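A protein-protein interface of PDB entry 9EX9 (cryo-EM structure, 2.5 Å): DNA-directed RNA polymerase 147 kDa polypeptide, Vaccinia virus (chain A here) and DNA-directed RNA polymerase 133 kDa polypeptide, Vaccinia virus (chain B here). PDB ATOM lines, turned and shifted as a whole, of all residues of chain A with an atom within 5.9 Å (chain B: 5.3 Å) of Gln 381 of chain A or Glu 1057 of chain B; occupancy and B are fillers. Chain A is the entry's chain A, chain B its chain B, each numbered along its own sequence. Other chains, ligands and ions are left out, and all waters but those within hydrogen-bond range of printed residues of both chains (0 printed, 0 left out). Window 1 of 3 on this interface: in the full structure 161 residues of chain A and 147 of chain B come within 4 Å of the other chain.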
ATOM      1  N   GLY A 379      16.567 -27.647   3.633  1.00  0.00           N
ATOM      2  CA  GLY A 379      17.765 -28.349   3.215  1.00  0.00           C
ATOM      3  C   GLY A 379      18.954 -27.431   3.057  1.00  0.00           C
ATOM      4  O   GLY A 379      18.896 -26.229   3.335  1.00  0.00           O
ATOM      5  N   ARG A 380      20.047 -28.044   2.606  1.00  0.00           N
ATOM      6  CA  ARG A 380      21.325 -27.389   2.369  1.00  0.00           C
ATOM      7  C   ARG A 380      21.775 -27.699   0.950  1.00  0.00           C
ATOM      8  O   ARG A 380      21.429 -28.748   0.401  1.00  0.00           O
ATOM      9  CB  ARG A 380      22.378 -27.866   3.370  1.00  0.00           C
ATOM     10  CG  ARG A 380      23.740 -27.232   3.195  1.00  0.00           C
ATOM     11  CD  ARG A 380      24.709 -27.688   4.266  1.00  0.00           C
ATOM     12  NE  ARG A 380      26.062 -27.218   4.006  1.00  0.00           N
ATOM     13  CZ  ARG A 380      26.897 -27.781   3.144  1.00  0.00           C
ATOM     14  NH1 ARG A 380      26.548 -28.840   2.435  1.00  0.00           N
ATOM     15  NH2 ARG A 380      28.111 -27.265   2.988  1.00  0.00           N
ATOM     16  N   GLN A 381      22.537 -26.782   0.353  1.00  0.00           N
ATOM     17  CA  GLN A 381      23.038 -26.978  -0.998  1.00  0.00           C
ATOM     18  C   GLN A 381      24.560 -27.061  -1.002  1.00  0.00           C
ATOM     19  O   GLN A 381      25.223 -26.400  -0.197  1.00  0.00           O
ATOM     20  CB  GLN A 381      22.599 -25.839  -1.922  1.00  0.00           C
ATOM     21  CG  GLN A 381      21.152 -25.911  -2.342  1.00  0.00           C
ATOM     22  CD  GLN A 381      20.720 -24.692  -3.119  1.00  0.00           C
ATOM     23  OE1 GLN A 381      21.060 -23.567  -2.762  1.00  0.00           O
ATOM     24  NE2 GLN A 381      19.970 -24.907  -4.189  1.00  0.00           N
ATOM     25  N   PRO A 382      25.155 -27.845  -1.909  1.00  0.00           N
ATOM     26  CA  PRO A 382      24.539 -28.628  -2.989  1.00  0.00           C
ATOM     27  C   PRO A 382      23.846 -29.888  -2.493  1.00  0.00           C
ATOM     28  O   PRO A 382      24.324 -30.551  -1.583  1.00  0.00           O
ATOM     29  CB  PRO A 382      25.735 -28.959  -3.884  1.00  0.00           C
ATOM     30  CG  PRO A 382      26.873 -29.069  -2.934  1.00  0.00           C
ATOM     31  CD  PRO A 382      26.617 -28.016  -1.890  1.00  0.00           C
ATOM     32  N   SER A 383      22.717 -30.247  -3.095  1.00  0.00           N
ATOM     33  CA  SER A 383      21.935 -31.403  -2.668  1.00  0.00           C
ATOM     34  C   SER A 383      22.450 -32.622  -3.418  1.00  0.00           C
ATOM     35  O   SER A 383      21.974 -32.960  -4.501  1.00  0.00           O
ATOM     36  CB  SER A 383      20.455 -31.165  -2.919  1.00  0.00           C
ATOM     37  OG  SER A 383      20.014 -30.011  -2.226  1.00  0.00           O
ATOM     38  N   ASN A 388      19.763 -34.410   1.871  1.00  0.00           N
ATOM     39  CA  ASN A 388      19.966 -32.972   1.939  1.00  0.00           C
ATOM     40  C   ASN A 388      18.660 -32.193   1.988  1.00  0.00           C
ATOM     41  O   ASN A 388      18.687 -31.005   2.324  1.00  0.00           O
ATOM     42  CB  ASN A 388      20.793 -32.504   0.743  1.00  0.00           C
ATOM     43  CG  ASN A 388      22.265 -32.752   0.928  1.00  0.00           C
ATOM     44  OD1 ASN A 388      22.793 -33.765   0.486  1.00  0.00           O
ATOM     45  ND2 ASN A 388      22.941 -31.826   1.588  1.00  0.00           N
ATOM     46  N   VAL A 389      17.530 -32.823   1.673  1.00  0.00           N
ATOM     47  CA  VAL A 389      16.225 -32.169   1.660  1.00  0.00           C
ATOM     48  C   VAL A 389      15.264 -33.023   2.475  1.00  0.00           C
ATOM     49  O   VAL A 389      14.995 -34.171   2.106  1.00  0.00           O
ATOM     50  CB  VAL A 389      15.698 -31.987   0.227  1.00  0.00           C
ATOM     51  CG1 VAL A 389      14.457 -31.119   0.219  1.00  0.00           C
ATOM     52  CG2 VAL A 389      16.773 -31.398  -0.658  1.00  0.00           C
ATOM     53  N   GLU A 420      24.673 -21.900   5.286  1.00  0.00           N
ATOM     54  CA  GLU A 420      23.305 -21.416   5.190  1.00  0.00           C
ATOM     55  C   GLU A 420      22.398 -22.546   4.732  1.00  0.00           C
ATOM     56  O   GLU A 420      22.849 -23.530   4.147  1.00  0.00           O
ATOM     57  CB  GLU A 420      23.189 -20.243   4.218  1.00  0.00           C
ATOM     58  CG  GLU A 420      23.984 -19.023   4.620  1.00  0.00           C
ATOM     59  CD  GLU A 420      23.855 -17.895   3.622  1.00  0.00           C
ATOM     60  OE1 GLU A 420      23.021 -18.011   2.701  1.00  0.00           O
ATOM     61  OE2 GLU A 420      24.586 -16.894   3.753  1.00  0.00           O
ATOM     62  N   TRP A 422      18.023 -23.394   3.397  1.00  0.00           N
ATOM     63  CA  TRP A 422      16.822 -22.835   2.796  1.00  0.00           C
ATOM     64  C   TRP A 422      15.591 -23.636   3.200  1.00  0.00           C
ATOM     65  O   TRP A 422      15.682 -24.820   3.543  1.00  0.00           O
ATOM     66  CB  TRP A 422      16.934 -22.795   1.274  1.00  0.00           C
ATOM     67  CG  TRP A 422      17.042 -24.138   0.656  1.00  0.00           C
ATOM     68  CD1 TRP A 422      18.182 -24.832   0.404  1.00  0.00           C
ATOM     69  CD2 TRP A 422      15.964 -24.958   0.207  1.00  0.00           C
ATOM     70  NE1 TRP A 422      17.882 -26.037  -0.173  1.00  0.00           N
ATOM     71  CE2 TRP A 422      16.524 -26.138  -0.304  1.00  0.00           C
ATOM     72  CE3 TRP A 422      14.577 -24.811   0.192  1.00  0.00           C
ATOM     73  CZ2 TRP A 422      15.749 -27.161  -0.828  1.00  0.00           C
ATOM     74  CZ3 TRP A 422      13.813 -25.827  -0.327  1.00  0.00           C
ATOM     75  CH2 TRP A 422      14.398 -26.986  -0.830  1.00  0.00           C
ATOM     76  N   LYS B1052      15.277 -19.980  -5.369  1.00  0.00           N
ATOM     77  CA  LYS B1052      15.101 -20.851  -6.523  1.00  0.00           C
ATOM     78  C   LYS B1052      15.126 -22.316  -6.108  1.00  0.00           C
ATOM     79  O   LYS B1052      16.032 -22.754  -5.394  1.00  0.00           O
ATOM     80  CB  LYS B1052      16.181 -20.595  -7.572  1.00  0.00           C
ATOM     81  CG  LYS B1052      15.982 -21.412  -8.832  1.00  0.00           C
ATOM     82  CD  LYS B1052      17.057 -21.143  -9.851  1.00  0.00           C
ATOM     83  CE  LYS B1052      16.972 -22.121 -11.004  1.00  0.00           C
ATOM     84  NZ  LYS B1052      17.981 -21.836 -12.056  1.00  0.00           N
ATOM     85  N   PHE B1053      14.134 -23.066  -6.574  1.00  0.00           N
ATOM     86  CA  PHE B1053      14.049 -24.507  -6.360  1.00  0.00           C
ATOM     87  C   PHE B1053      14.716 -25.185  -7.550  1.00  0.00           C
ATOM     88  O   PHE B1053      14.109 -25.340  -8.609  1.00  0.00           O
ATOM     89  CB  PHE B1053      12.591 -24.925  -6.206  1.00  0.00           C
ATOM     90  CG  PHE B1053      12.400 -26.362  -5.823  1.00  0.00           C
ATOM     91  CD1 PHE B1053      12.360 -26.737  -4.495  1.00  0.00           C
ATOM     92  CD2 PHE B1053      12.245 -27.337  -6.789  1.00  0.00           C
ATOM     93  CE1 PHE B1053      12.184 -28.055  -4.142  1.00  0.00           C
ATOM     94  CE2 PHE B1053      12.068 -28.654  -6.438  1.00  0.00           C
ATOM     95  CZ  PHE B1053      12.038 -29.013  -5.115  1.00  0.00           C
ATOM     96  N   GLY B1054      15.969 -25.588  -7.384  1.00  0.00           N
ATOM     97  CA  GLY B1054      16.722 -26.146  -8.486  1.00  0.00           C
ATOM     98  C   GLY B1054      16.318 -27.571  -8.797  1.00  0.00           C
ATOM     99  O   GLY B1054      15.545 -28.203  -8.083  1.00  0.00           O
ATOM    100  N   GLU B1055      16.864 -28.094  -9.896  1.00  0.00           N
ATOM    101  CA  GLU B1055      16.501 -29.441 -10.324  1.00  0.00           C
ATOM    102  C   GLU B1055      17.245 -30.530  -9.561  1.00  0.00           C
ATOM    103  O   GLU B1055      16.839 -31.694  -9.620  1.00  0.00           O
ATOM    104  CB  GLU B1055      16.738 -29.609 -11.824  1.00  0.00           C
ATOM    105  CG  GLU B1055      18.157 -29.395 -12.273  1.00  0.00           C
ATOM    106  CD  GLU B1055      18.370 -29.818 -13.708  1.00  0.00           C
ATOM    107  OE1 GLU B1055      17.459 -30.449 -14.282  1.00  0.00           O
ATOM    108  OE2 GLU B1055      19.448 -29.524 -14.265  1.00  0.00           O
ATOM    109  N   MET B1056      18.310 -30.190  -8.837  1.00  0.00           N
ATOM    110  CA  MET B1056      18.903 -31.157  -7.922  1.00  0.00           C
ATOM    111  C   MET B1056      17.987 -31.410  -6.728  1.00  0.00           C
ATOM    112  O   MET B1056      17.817 -32.558  -6.295  1.00  0.00           O
ATOM    113  CB  MET B1056      20.274 -30.664  -7.472  1.00  0.00           C
ATOM    114  CG  MET B1056      21.291 -30.623  -8.604  1.00  0.00           C
ATOM    115  SD  MET B1056      22.822 -29.778  -8.175  1.00  0.00           S
ATOM    116  CE  MET B1056      23.461 -30.844  -6.895  1.00  0.00           C
ATOM    117  N   GLU B1057      17.366 -30.356  -6.199  1.00  0.00           N
ATOM    118  CA  GLU B1057      16.331 -30.544  -5.190  1.00  0.00           C
ATOM    119  C   GLU B1057      15.174 -31.354  -5.753  1.00  0.00           C
ATOM    120  O   GLU B1057      14.569 -32.169  -5.048  1.00  0.00           O
ATOM    121  CB  GLU B1057      15.833 -29.194  -4.683  1.00  0.00           C
ATOM    122  CG  GLU B1057      16.825 -28.420  -3.846  1.00  0.00           C
ATOM    123  CD  GLU B1057      17.948 -27.830  -4.659  1.00  0.00           C
ATOM    124  OE1 GLU B1057      17.924 -27.983  -5.893  1.00  0.00           O
ATOM    125  OE2 GLU B1057      18.854 -27.211  -4.069  1.00  0.00           O
ATOM    126  N   ARG B1058      14.842 -31.134  -7.022  1.00  0.00           N
ATOM    127  CA  ARG B1058      13.783 -31.908  -7.654  1.00  0.00           C
ATOM    128  C   ARG B1058      14.151 -33.386  -7.707  1.00  0.00           C
ATOM    129  O   ARG B1058      13.312 -34.256  -7.434  1.00  0.00           O
ATOM    130  CB  ARG B1058      13.520 -31.349  -9.050  1.00  0.00           C
ATOM    131  CG  ARG B1058      12.289 -31.891  -9.740  1.00  0.00           C
ATOM    132  CD  ARG B1058      12.597 -33.098 -10.581  1.00  0.00           C
ATOM    133  NE  ARG B1058      13.631 -32.825 -11.565  1.00  0.00           N
ATOM    134  CZ  ARG B1058      14.210 -33.752 -12.312  1.00  0.00           C
ATOM    135  NH1 ARG B1058      13.881 -35.028 -12.210  1.00  0.00           N
ATOM    136  NH2 ARG B1058      15.143 -33.392 -13.184  1.00  0.00           N
ATOM    137  N   ASP B1059      15.407 -33.690  -8.041  1.00  0.00           N
ATOM    138  CA  ASP B1059      15.859 -35.076  -8.020  1.00  0.00           C
ATOM    139  C   ASP B1059      15.738 -35.662  -6.623  1.00  0.00           C
ATOM    140  O   ASP B1059      15.295 -36.802  -6.453  1.00  0.00           O
ATOM    141  CB  ASP B1059      17.306 -35.169  -8.500  1.00  0.00           C
ATOM    142  CG  ASP B1059      17.497 -34.631  -9.897  1.00  0.00           C
ATOM    143  OD1 ASP B1059      16.570 -34.758 -10.723  1.00  0.00           O
ATOM    144  OD2 ASP B1059      18.582 -34.085 -10.174  1.00  0.00           O
ATOM    145  N   CYS B1060      16.129 -34.893  -5.607  1.00  0.00           N
ATOM    146  CA  CYS B1060      16.037 -35.385  -4.238  1.00  0.00           C
ATOM    147  C   CYS B1060      14.596 -35.714  -3.872  1.00  0.00           C
ATOM    148  O   CYS B1060      14.314 -36.771  -3.301  1.00  0.00           O
ATOM    149  CB  CYS B1060      16.613 -34.356  -3.270  1.00  0.00           C
ATOM    150  SG  CYS B1060      18.393 -34.158  -3.385  1.00  0.00           S
ATOM    151  N   LEU B1061      13.664 -34.824  -4.209  1.00  0.00           N
ATOM    152  CA  LEU B1061      12.264 -35.066  -3.869  1.00  0.00           C
ATOM    153  C   LEU B1061      11.717 -36.275  -4.611  1.00  0.00           C
ATOM    154  O   LEU B1061      10.871 -37.002  -4.085  1.00  0.00           O
ATOM    155  CB  LEU B1061      11.415 -33.834  -4.175  1.00  0.00           C
ATOM    156  CG  LEU B1061      10.677 -33.241  -2.977  1.00  0.00           C
ATOM    157  CD1 LEU B1061      11.664 -32.711  -1.968  1.00  0.00           C
ATOM    158  CD2 LEU B1061       9.745 -32.149  -3.423  1.00  0.00           C
ATOM    159  N   ILE B1062      12.166 -36.495  -5.846  1.00  0.00           N
ATOM    160  CA  ILE B1062      11.755 -37.706  -6.551  1.00  0.00           C
ATOM    161  C   ILE B1062      12.376 -38.942  -5.909  1.00  0.00           C
ATOM    162  O   ILE B1062      11.817 -40.040  -6.002  1.00  0.00           O
ATOM    163  CB  ILE B1062      12.105 -37.596  -8.043  1.00  0.00           C
ATOM    164  CG1 ILE B1062      11.075 -36.705  -8.734  1.00  0.00           C
ATOM    165  CG2 ILE B1062      12.159 -38.974  -8.685  1.00  0.00           C
ATOM    166  CD1 ILE B1062      11.281 -36.546 -10.205  1.00  0.00           C
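Ser 383 of chain A touches Met 1056 of chain B (O to CE, 3.5 Å). Glu 1057 of chain B touches Ser 383 of chain A. SG of Cys 1060 of chain B touches CB of Ser 383 of chain A, at 3.7 Å. CG2 of Val 389 of chain A touches CB of Cys 1060 of chain B, 3.9 Å away. CD1 of Leu 1061 of chain B touches CG1 of Val 389 of chain A, at 3.9 Å. CG of Glu 1057 of chain B touches CZ2 of Trp 422 of chain A, 3.4 Å away.
The backbone carbonyl oxygen (O) of Trp 422 of chain A is in hydrogen-bond range of the backbone NH (N) of Gly 379 of chain A. OG of Ser 383 of chain A lies within hydrogen-bond range of O of Arg 380 of chain A (3.2 Å). The side-chain carboxylate (OE1) of Glu 1057 of chain B lies close to the backbone NH (N) of Gly 1054 of chain B (3.4 Å). The backbone carbonyl oxygen (O) of Met 1056 of chain B lies within hydrogen-bond range of the side-chain sulfur (SG) of Cys 1060 of chain B (3.4 Å).
Of chain B, only Glu 1057 (2.6 Å) comes within 4 Å of Gln 381 of chain A. Glu 1057 of chain B touches just these residues of chain A: Gln 381 (2.6 Å), Ser 383 (3.5 Å) and Trp 422 (3.4 Å). Of the printed residues of chain A, Cys 1060 of chain B touches Ser 383 and Val 389. Printed residues of chain A within 4 Å of Met 1056 of chain B: Ser 383. Of the printed residues of chain B, Ser 383 of chain A touches Met 1056, Glu 1057 and Cys 1060. Printed residues of chain B within 4 Å of Trp 422 of chain A: Glu 1057 (3.4 Å). Of the printed residues of chain A, Leu 1061 of chain B touches Val 389. Arg 1058 of chain B touches none of the printed residues of chain A. The nearest residue of chain A that does not touch Glu 1057 of chain B is Val 389 of chain A (4.4 Å).
Printed residues of chain A that touch a printed residue of chain B: Gln 381, Ser 383, Val 389 and Trp 422. Hydrophobic or aromatic side chains of chain A that line the printed part of chain B: Val 389 and Trp 422. Hydrophobic or aromatic side chains of chain B within 4 Å of the printed part of chain A: Met 1056 and Leu 1061. Among the printed residues, no Asp or Glu carboxylate lies within 4 Å of a Lys or Arg side-chain nitrogen of the other chain.
The side-chain carboxylate (OE2) of Glu 1057 of chain B sits at hydrogen-bond distance from the side-chain amide nitrogen (NE2) of Gln 381 of chain A, 2.6 Å away.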
